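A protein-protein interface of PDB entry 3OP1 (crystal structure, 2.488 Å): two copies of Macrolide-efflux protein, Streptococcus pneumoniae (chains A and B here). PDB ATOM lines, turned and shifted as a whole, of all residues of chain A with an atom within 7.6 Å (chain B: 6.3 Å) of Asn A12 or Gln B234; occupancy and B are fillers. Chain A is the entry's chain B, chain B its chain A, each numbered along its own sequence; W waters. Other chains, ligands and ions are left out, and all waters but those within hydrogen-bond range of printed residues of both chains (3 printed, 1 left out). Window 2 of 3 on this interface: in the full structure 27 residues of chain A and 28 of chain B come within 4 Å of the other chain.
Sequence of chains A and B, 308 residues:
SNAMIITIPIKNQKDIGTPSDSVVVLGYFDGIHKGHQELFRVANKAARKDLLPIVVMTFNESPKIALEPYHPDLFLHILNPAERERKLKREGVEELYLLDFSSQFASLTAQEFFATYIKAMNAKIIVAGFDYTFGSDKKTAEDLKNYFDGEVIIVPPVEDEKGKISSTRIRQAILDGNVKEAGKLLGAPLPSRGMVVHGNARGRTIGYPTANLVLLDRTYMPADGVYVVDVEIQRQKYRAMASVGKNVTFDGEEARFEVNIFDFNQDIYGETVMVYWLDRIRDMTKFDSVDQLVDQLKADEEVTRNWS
The side-chain amide nitrogen (NE2) of Gln B234 is in hydrogen-bond range of the side-chain carboxylate (OE2) of Glu B271, 3.1 Å away.
The backbone NH (N) of Lys A11 lies within hydrogen-bond range of the side-chain carboxylate (OD2) of Asp A15 (3.2 Å).
The side-chain amide oxygen of Asn A12 lies close to the backbone NH of Lys A14.
The side-chain amide oxygen (OD1) of Asn A12 sits close to the side-chain carboxylate (OD2) of Asp A15, at 3.4 Å.
Of the printed residues of chain B, Asn A12 touches Gln B234.
Of the printed residues of chain B, Asp A15 touches Arg B235.
Tyr A97 touches none of the printed residues of chain B.
Of the printed residues of chain B, Asp A100 touches Thr B272.
Of the printed residues of chain A, Arg B235 touches Lys A11 (3.1 Å) and Asp A15 (3.0 Å).
Of the printed residues of chain A, Thr B272 touches Asp A100.
The nearest printed residue of chain B that does not touch Asn A12 is Arg B235 (5.0 Å).
The nearest printed residue of chain A that does not touch Thr B272 is Lys A11 (4.2 Å).
No position is printed for both chains.
Of the 6 pairs that touch across the chains among the printed residues, none has its exchanged pair printed and touching as well.
Of the 8 printed residues of chain B, 4 touch a printed residue of chain A.
Printed residues of chain B that touch a printed residue of chain A: Gln B234, Arg B235, Glu B271 and Thr B272.
Among the printed residues, 6 pairs touch across the chains.
Among the printed residues, Asp or Glu carboxylates within 4 Å of a Lys or Arg side-chain nitrogen of the other chain: Asp A15 with Arg B235 (3.0 Å).
Among the printed residues, merely in contact across the chains: Lys A11 with Arg B235 (3.1 Å), Ser A102 with Glu B271 (3.4 Å), Lys A11 with Gln B234 (3.5 Å) and Asn A12 with Gln B234 (3.98 Å).
The guanidinium group (NH2) of Arg B235 lies within salt-bridge range of the side-chain carboxylate (OD2) of Asp A15 (3.0 Å).
The side-chain carboxylate (OD2) of Asp A100 is in hydrogen-bond range of the side-chain hydroxyl (OG1) of Thr B272.
Water W2 lies within hydrogen-bond range of OG of Ser A102 (2.6 Å), O of Asp A100 (3.0 Å) and OE2 of Glu B271 (3.3 Å).
Water W1 lies within hydrogen-bond range of the backbone NH (N) of Gln B234, the backbone carbonyl oxygen (O) of Thr B272, the side-chain amino group (NZ) of Lys A11 and the side-chain carboxylate (OE2) of Glu B271.
Water W3 lies within hydrogen-bond range of N of Gln A104 (2.8 Å), OG of Ser A102 (3.3 Å) and OE1 of Glu B271 (3.3 Å).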
ATOM      1  N   PRO A   9      16.819  -3.946  10.490  1.00  0.00           N
ATOM      2  CA  PRO A   9      16.625  -3.466   9.116  1.00  0.00           C
ATOM      3  C   PRO A   9      15.193  -3.702   8.650  1.00  0.00           C
ATOM      4  O   PRO A   9      14.570  -4.719   8.944  1.00  0.00           O
ATOM      5  CB  PRO A   9      17.583  -4.347   8.288  1.00  0.00           C
ATOM      6  CG  PRO A   9      17.497  -5.660   8.991  1.00  0.00           C
ATOM      7  CD  PRO A   9      17.420  -5.293  10.501  1.00  0.00           C
ATOM      8  N   ILE A  10      14.646  -2.697   7.992  1.00  0.00           N
ATOM      9  CA  ILE A  10      13.270  -2.746   7.575  1.00  0.00           C
ATOM     10  C   ILE A  10      13.085  -2.259   6.149  1.00  0.00           C
ATOM     11  O   ILE A  10      13.709  -1.292   5.729  1.00  0.00           O
ATOM     12  CB  ILE A  10      12.411  -1.882   8.513  1.00  0.00           C
ATOM     13  CG1 ILE A  10      12.998  -0.482   8.620  1.00  0.00           C
ATOM     14  CG2 ILE A  10      12.361  -2.494   9.890  1.00  0.00           C
ATOM     15  CD1 ILE A  10      11.995   0.609   8.490  1.00  0.00           C
ATOM     16  N   LYS A  11      12.255  -2.964   5.395  1.00  0.00           N
ATOM     17  CA  LYS A  11      11.798  -2.494   4.102  1.00  0.00           C
ATOM     18  C   LYS A  11      10.849  -1.309   4.263  1.00  0.00           C
ATOM     19  O   LYS A  11      10.859  -0.371   3.477  1.00  0.00           O
ATOM     20  CB  LYS A  11      11.149  -3.622   3.315  1.00  0.00           C
ATOM     21  CG  LYS A  11      11.864  -4.947   3.455  1.00  0.00           C
ATOM     22  CD  LYS A  11      13.104  -5.008   2.589  1.00  0.00           C
ATOM     23  CE  LYS A  11      13.363  -3.688   1.901  1.00  0.00           C
ATOM     24  NZ  LYS A  11      14.435  -3.798   0.881  1.00  0.00           N
ATOM     25  N   ASN A  12      10.009  -1.388   5.288  1.00  0.00           N
ATOM     26  CA  ASN A  12       8.986  -0.380   5.557  1.00  0.00           C
ATOM     27  C   ASN A  12       8.500  -0.350   7.004  1.00  0.00           C
ATOM     28  O   ASN A  12       8.921  -1.151   7.829  1.00  0.00           O
ATOM     29  CB  ASN A  12       7.811  -0.479   4.579  1.00  0.00           C
ATOM     30  CG  ASN A  12       7.060  -1.785   4.684  1.00  0.00           C
ATOM     31  OD1 ASN A  12       7.202  -2.530   5.642  1.00  0.00           O
ATOM     32  ND2 ASN A  12       6.249  -2.067   3.686  1.00  0.00           N
ATOM     33  N   GLN A  13       7.599   0.578   7.292  1.00  0.00           N
ATOM     34  CA  GLN A  13       7.084   0.807   8.638  1.00  0.00           C
ATOM     35  C   GLN A  13       6.386  -0.401   9.248  1.00  0.00           C
ATOM     36  O   GLN A  13       6.362  -0.561  10.459  1.00  0.00           O
ATOM     37  CB  GLN A  13       6.139   2.001   8.638  1.00  0.00           C
ATOM     38  CG  GLN A  13       5.741   2.472   7.261  1.00  0.00           C
ATOM     39  CD  GLN A  13       4.610   1.665   6.690  1.00  0.00           C
ATOM     40  OE1 GLN A  13       4.339   0.560   7.137  1.00  0.00           O
ATOM     41  NE2 GLN A  13       3.939   2.216   5.700  1.00  0.00           N
ATOM     42  N   LYS A  14       5.811  -1.245   8.407  1.00  0.00           N
ATOM     43  CA  LYS A  14       5.118  -2.442   8.863  1.00  0.00           C
ATOM     44  C   LYS A  14       6.078  -3.345   9.613  1.00  0.00           C
ATOM     45  O   LYS A  14       5.682  -4.089  10.490  1.00  0.00           O
ATOM     46  CB  LYS A  14       4.522  -3.201   7.685  1.00  0.00           C
ATOM     47  CG  LYS A  14       3.041  -3.011   7.517  1.00  0.00           C
ATOM     48  CD  LYS A  14       2.725  -2.223   6.272  1.00  0.00           C
ATOM     49  CE  LYS A  14       1.338  -2.537   5.771  1.00  0.00           C
ATOM     50  NZ  LYS A  14       0.897  -3.886   6.204  1.00  0.00           N
ATOM     51  N   ASP A  15       7.337  -3.314   9.216  1.00  0.00           N
ATOM     52  CA  ASP A  15       8.378  -4.120   9.843  1.00  0.00           C
ATOM     53  C   ASP A  15       8.739  -3.721  11.277  1.00  0.00           C
ATOM     54  O   ASP A  15       9.319  -4.509  12.012  1.00  0.00           O
ATOM     55  CB  ASP A  15       9.618  -4.156   8.957  1.00  0.00           C
ATOM     56  CG  ASP A  15       9.408  -4.980   7.711  1.00  0.00           C
ATOM     57  OD1 ASP A  15       8.899  -6.108   7.819  1.00  0.00           O
ATOM     58  OD2 ASP A  15       9.750  -4.498   6.622  1.00  0.00           O
ATOM     59  N   ILE A  16       8.427  -2.484  11.646  1.00  0.00           N
ATOM     60  CA  ILE A  16       8.790  -1.917  12.943  1.00  0.00           C
ATOM     61  C   ILE A  16       7.985  -2.641  13.999  1.00  0.00           C
ATOM     62  O   ILE A  16       6.871  -3.047  13.740  1.00  0.00           O
ATOM     63  CB  ILE A  16       8.515  -0.398  13.007  1.00  0.00           C
ATOM     64  CG1 ILE A  16       9.510   0.361  12.110  1.00  0.00           C
ATOM     65  CG2 ILE A  16       8.622   0.082  14.443  1.00  0.00           C
ATOM     66  CD1 ILE A  16       9.138   1.802  11.812  1.00  0.00           C
ATOM     67  N   GLY A  17       8.602  -2.906  15.139  1.00  0.00           N
ATOM     68  CA  GLY A  17       7.951  -3.671  16.181  1.00  0.00           C
ATOM     69  C   GLY A  17       7.922  -3.125  17.590  1.00  0.00           C
ATOM     70  O   GLY A  17       7.736  -3.904  18.516  1.00  0.00           O
ATOM     71  N   TYR A  97      16.349   1.386  13.846  1.00  0.00           N
ATOM     72  CA  TYR A  97      15.834   0.923  12.567  1.00  0.00           C
ATOM     73  C   TYR A  97      16.649   1.461  11.398  1.00  0.00           C
ATOM     74  O   TYR A  97      16.944   2.654  11.328  1.00  0.00           O
ATOM     75  CB  TYR A  97      14.344   1.269  12.447  1.00  0.00           C
ATOM     76  CG  TYR A  97      13.486   0.537  13.476  1.00  0.00           C
ATOM     77  CD1 TYR A  97      13.178  -0.826  13.318  1.00  0.00           C
ATOM     78  CD2 TYR A  97      12.994   1.206  14.621  1.00  0.00           C
ATOM     79  CE1 TYR A  97      12.409  -1.505  14.265  1.00  0.00           C
ATOM     80  CE2 TYR A  97      12.209   0.541  15.585  1.00  0.00           C
ATOM     81  CZ  TYR A  97      11.916  -0.819  15.403  1.00  0.00           C
ATOM     82  OH  TYR A  97      11.144  -1.501  16.332  1.00  0.00           O
ATOM     83  N   LEU A  98      16.998   0.574  10.481  1.00  0.00           N
ATOM     84  CA  LEU A  98      17.714   0.970   9.284  1.00  0.00           C
ATOM     85  C   LEU A  98      16.847   0.728   8.067  1.00  0.00           C
ATOM     86  O   LEU A  98      16.356  -0.360   7.840  1.00  0.00           O
ATOM     87  CB  LEU A  98      19.030   0.221   9.194  1.00  0.00           C
ATOM     88  CG  LEU A  98      19.856   0.498  10.445  1.00  0.00           C
ATOM     89  CD1 LEU A  98      20.917  -0.545  10.677  1.00  0.00           C
ATOM     90  CD2 LEU A  98      20.439   1.892  10.398  1.00  0.00           C
ATOM     91  N   LEU A  99      16.663   1.777   7.290  1.00  0.00           N
ATOM     92  CA  LEU A  99      15.801   1.737   6.138  1.00  0.00           C
ATOM     93  C   LEU A  99      16.525   2.401   4.992  1.00  0.00           C
ATOM     94  O   LEU A  99      17.385   3.237   5.206  1.00  0.00           O
ATOM     95  CB  LEU A  99      14.505   2.486   6.445  1.00  0.00           C
ATOM     96  CG  LEU A  99      13.680   2.997   5.268  1.00  0.00           C
ATOM     97  CD1 LEU A  99      12.497   2.112   5.042  1.00  0.00           C
ATOM     98  CD2 LEU A  99      13.250   4.421   5.452  1.00  0.00           C
ATOM     99  N   ASP A 100      16.186   2.023   3.772  1.00  0.00           N
ATOM    100  CA  ASP A 100      16.796   2.643   2.618  1.00  0.00           C
ATOM    101  C   ASP A 100      16.053   3.908   2.286  1.00  0.00           C
ATOM    102  O   ASP A 100      14.842   3.907   2.207  1.00  0.00           O
ATOM    103  CB  ASP A 100      16.770   1.708   1.419  1.00  0.00           C
ATOM    104  CG  ASP A 100      17.698   0.546   1.578  1.00  0.00           C
ATOM    105  OD1 ASP A 100      18.852   0.770   1.971  1.00  0.00           O
ATOM    106  OD2 ASP A 100      17.274  -0.594   1.313  1.00  0.00           O
ATOM    107  N   SER A 102      14.724   5.466  -0.064  1.00  0.00           N
ATOM    108  CA  SER A 102      14.253   5.264  -1.421  1.00  0.00           C
ATOM    109  C   SER A 102      13.521   6.472  -1.961  1.00  0.00           C
ATOM    110  O   SER A 102      13.220   7.393  -1.233  1.00  0.00           O
ATOM    111  CB  SER A 102      13.363   4.031  -1.499  1.00  0.00           C
ATOM    112  OG  SER A 102      12.218   4.173  -0.695  1.00  0.00           O
ATOM    113  N   GLN A 104      10.586   6.414  -2.937  1.00  0.00           N
ATOM    114  CA  GLN A 104       9.297   6.312  -2.283  1.00  0.00           C
ATOM    115  C   GLN A 104       9.295   6.968  -0.909  1.00  0.00           C
ATOM    116  O   GLN A 104       8.376   7.688  -0.560  1.00  0.00           O
ATOM    117  CB  GLN A 104       8.880   4.857  -2.150  1.00  0.00           C
ATOM    118  CG  GLN A 104       7.776   4.633  -1.137  1.00  0.00           C
ATOM    119  CD  GLN A 104       7.021   3.353  -1.428  1.00  0.00           C
ATOM    120  OE1 GLN A 104       7.314   2.673  -2.417  1.00  0.00           O
ATOM    121  NE2 GLN A 104       6.054   3.012  -0.582  1.00  0.00           N
ATOM    122  N   THR A 116       2.740   6.850   9.173  1.00  0.00           N
ATOM    123  CA  THR A 116       3.332   5.541   8.985  1.00  0.00           C
ATOM    124  C   THR A 116       4.371   5.248  10.025  1.00  0.00           C
ATOM    125  O   THR A 116       4.135   4.444  10.925  1.00  0.00           O
ATOM    126  CB  THR A 116       3.988   5.446   7.628  1.00  0.00           C
ATOM    127  OG1 THR A 116       4.809   6.604   7.435  1.00  0.00           O
ATOM    128  CG2 THR A 116       2.924   5.400   6.567  1.00  0.00           C
ATOM    129  N   TYR A 117       5.522   5.897   9.904  1.00  0.00           N
ATOM    130  CA  TYR A 117       6.660   5.485  10.701  1.00  0.00           C
ATOM    131  C   TYR A 117       6.517   5.914  12.172  1.00  0.00           C
ATOM    132  O   TYR A 117       6.734   5.100  13.085  1.00  0.00           O
ATOM    133  CB  TYR A 117       8.003   5.904  10.046  1.00  0.00           C
ATOM    134  CG  TYR A 117       8.304   5.145   8.751  1.00  0.00           C
ATOM    135  CD1 TYR A 117       8.882   3.879   8.780  1.00  0.00           C
ATOM    136  CD2 TYR A 117       7.991   5.687   7.491  1.00  0.00           C
ATOM    137  CE1 TYR A 117       9.143   3.168   7.598  1.00  0.00           C
ATOM    138  CE2 TYR A 117       8.253   4.978   6.294  1.00  0.00           C
ATOM    139  CZ  TYR A 117       8.833   3.706   6.357  1.00  0.00           C
ATOM    140  OH  TYR A 117       9.097   2.952   5.193  1.00  0.00           O
ATOM    141  N   ALA A 120       4.071   3.749  13.845  1.00  0.00           N
ATOM    142  CA  ALA A 120       4.642   2.442  14.090  1.00  0.00           C
ATOM    143  C   ALA A 120       5.567   2.533  15.277  1.00  0.00           C
ATOM    144  O   ALA A 120       5.672   1.602  16.068  1.00  0.00           O
ATOM    145  CB  ALA A 120       5.381   1.966  12.875  1.00  0.00           C
ATOM    146  N   GLU B 232      14.120  -8.677  -7.037  1.00  0.00           N
ATOM    147  CA  GLU B 232      13.231  -8.505  -5.900  1.00  0.00           C
ATOM    148  C   GLU B 232      13.246  -7.097  -5.331  1.00  0.00           C
ATOM    149  O   GLU B 232      14.249  -6.638  -4.821  1.00  0.00           O
ATOM    150  CB  GLU B 232      13.595  -9.488  -4.804  1.00  0.00           C
ATOM    151  CG  GLU B 232      12.485  -9.720  -3.820  1.00  0.00           C
ATOM    152  CD  GLU B 232      12.959 -10.419  -2.576  1.00  0.00           C
ATOM    153  OE1 GLU B 232      13.377  -9.723  -1.634  1.00  0.00           O
ATOM    154  OE2 GLU B 232      12.913 -11.662  -2.539  1.00  0.00           O
ATOM    155  N   ILE B 233      12.102  -6.430  -5.403  1.00  0.00           N
ATOM    156  CA  ILE B 233      11.939  -5.104  -4.848  1.00  0.00           C
ATOM    157  C   ILE B 233      10.770  -5.092  -3.888  1.00  0.00           C
ATOM    158  O   ILE B 233       9.661  -5.453  -4.249  1.00  0.00           O
ATOM    159  CB  ILE B 233      11.650  -4.089  -5.939  1.00  0.00           C
ATOM    160  CG1 ILE B 233      12.388  -4.470  -7.215  1.00  0.00           C
ATOM    161  CG2 ILE B 233      12.033  -2.700  -5.482  1.00  0.00           C
ATOM    162  CD1 ILE B 233      11.706  -4.007  -8.456  1.00  0.00           C
ATOM    163  N   GLN B 234      11.024  -4.670  -2.661  1.00  0.00           N
ATOM    164  CA  GLN B 234       9.982  -4.590  -1.666  1.00  0.00           C
ATOM    165  C   GLN B 234       9.281  -5.924  -1.540  1.00  0.00           C
ATOM    166  O   GLN B 234       8.075  -5.980  -1.412  1.00  0.00           O
ATOM    167  CB  GLN B 234       8.991  -3.491  -2.014  1.00  0.00           C
ATOM    168  CG  GLN B 234       9.425  -2.108  -1.574  1.00  0.00           C
ATOM    169  CD  GLN B 234       9.772  -2.031  -0.101  1.00  0.00           C
ATOM    170  OE1 GLN B 234       8.948  -2.302   0.764  1.00  0.00           O
ATOM    171  NE2 GLN B 234      11.002  -1.648   0.187  1.00  0.00           N
ATOM    172  N   ARG B 235      10.043  -7.000  -1.594  1.00  0.00           N
ATOM    173  CA  ARG B 235       9.500  -8.332  -1.396  1.00  0.00           C
ATOM    174  C   ARG B 235       8.677  -8.848  -2.570  1.00  0.00           C
ATOM    175  O   ARG B 235       7.990  -9.851  -2.452  1.00  0.00           O
ATOM    176  CB  ARG B 235       8.672  -8.383  -0.118  1.00  0.00           C
ATOM    177  CG  ARG B 235       9.377  -7.832   1.099  1.00  0.00           C
ATOM    178  CD  ARG B 235       9.729  -8.931   2.074  1.00  0.00           C
ATOM    179  NE  ARG B 235      10.326  -8.410   3.297  1.00  0.00           N
ATOM    180  CZ  ARG B 235       9.780  -7.465   4.054  1.00  0.00           C
ATOM    181  NH1 ARG B 235       8.621  -6.924   3.721  1.00  0.00           N
ATOM    182  NH2 ARG B 235      10.399  -7.058   5.147  1.00  0.00           N
ATOM    183  N   GLN B 236       8.756  -8.168  -3.702  1.00  0.00           N
ATOM    184  CA  GLN B 236       8.045  -8.599  -4.894  1.00  0.00           C
ATOM    185  C   GLN B 236       9.054  -8.914  -5.983  1.00  0.00           C
ATOM    186  O   GLN B 236       9.946  -8.122  -6.248  1.00  0.00           O
ATOM    187  CB  GLN B 236       7.078  -7.517  -5.373  1.00  0.00           C
ATOM    188  CG  GLN B 236       5.784  -7.444  -4.595  1.00  0.00           C
ATOM    189  CD  GLN B 236       4.729  -8.377  -5.139  1.00  0.00           C
ATOM    190  OE1 GLN B 236       4.260  -9.270  -4.443  1.00  0.00           O
ATOM    191  NE2 GLN B 236       4.349  -8.172  -6.395  1.00  0.00           N
ATOM    192  N   TYR B 238      10.204  -9.530  -9.821  1.00  0.00           N
ATOM    193  CA  TYR B 238       9.892  -9.184 -11.197  1.00  0.00           C
ATOM    194  C   TYR B 238      10.873  -9.849 -12.143  1.00  0.00           C
ATOM    195  O   TYR B 238      12.047 -10.040 -11.819  1.00  0.00           O
ATOM    196  CB  TYR B 238       9.993  -7.667 -11.363  1.00  0.00           C
ATOM    197  CG  TYR B 238       9.054  -6.947 -10.435  1.00  0.00           C
ATOM    198  CD1 TYR B 238       7.825  -6.420 -10.898  1.00  0.00           C
ATOM    199  CD2 TYR B 238       9.362  -6.819  -9.084  1.00  0.00           C
ATOM    200  CE1 TYR B 238       6.942  -5.757 -10.019  1.00  0.00           C
ATOM    201  CE2 TYR B 238       8.494  -6.158  -8.195  1.00  0.00           C
ATOM    202  CZ  TYR B 238       7.292  -5.645  -8.663  1.00  0.00           C
ATOM    203  OH  TYR B 238       6.463  -5.025  -7.769  1.00  0.00           O
ATOM    204  N   GLU B 271      16.900   2.469  -3.537  1.00  0.00           N
ATOM    205  CA  GLU B 271      16.332   1.244  -3.030  1.00  0.00           C
ATOM    206  C   GLU B 271      17.298   0.050  -3.239  1.00  0.00           C
ATOM    207  O   GLU B 271      17.958  -0.099  -4.280  1.00  0.00           O
ATOM    208  CB  GLU B 271      15.006   1.014  -3.735  1.00  0.00           C
ATOM    209  CG  GLU B 271      14.207  -0.158  -3.235  1.00  0.00           C
ATOM    210  CD  GLU B 271      13.211   0.235  -2.194  1.00  0.00           C
ATOM    211  OE1 GLU B 271      12.231   0.982  -2.503  1.00  0.00           O
ATOM    212  OE2 GLU B 271      13.423  -0.214  -1.055  1.00  0.00           O
ATOM    213  N   THR B 272      17.395  -0.806  -2.242  1.00  0.00           N
ATOM    214  CA  THR B 272      18.189  -2.007  -2.392  1.00  0.00           C
ATOM    215  C   THR B 272      17.367  -3.027  -3.149  1.00  0.00           C
ATOM    216  O   THR B 272      16.194  -3.215  -2.838  1.00  0.00           O
ATOM    217  CB  THR B 272      18.596  -2.586  -1.004  1.00  0.00           C
ATOM    218  OG1 THR B 272      19.523  -1.698  -0.364  1.00  0.00           O
ATOM    219  CG2 THR B 272      19.255  -3.948  -1.145  1.00  0.00           C
HETATM  220  O   HOH W   1      13.324  -3.303  -1.912  1.00  0.00           O
HETATM  221  O   HOH W   2      12.676   2.255   1.016  1.00  0.00           O
HETATM  222  O   HOH W   3      11.287   3.869  -3.836  1.00  0.00           O
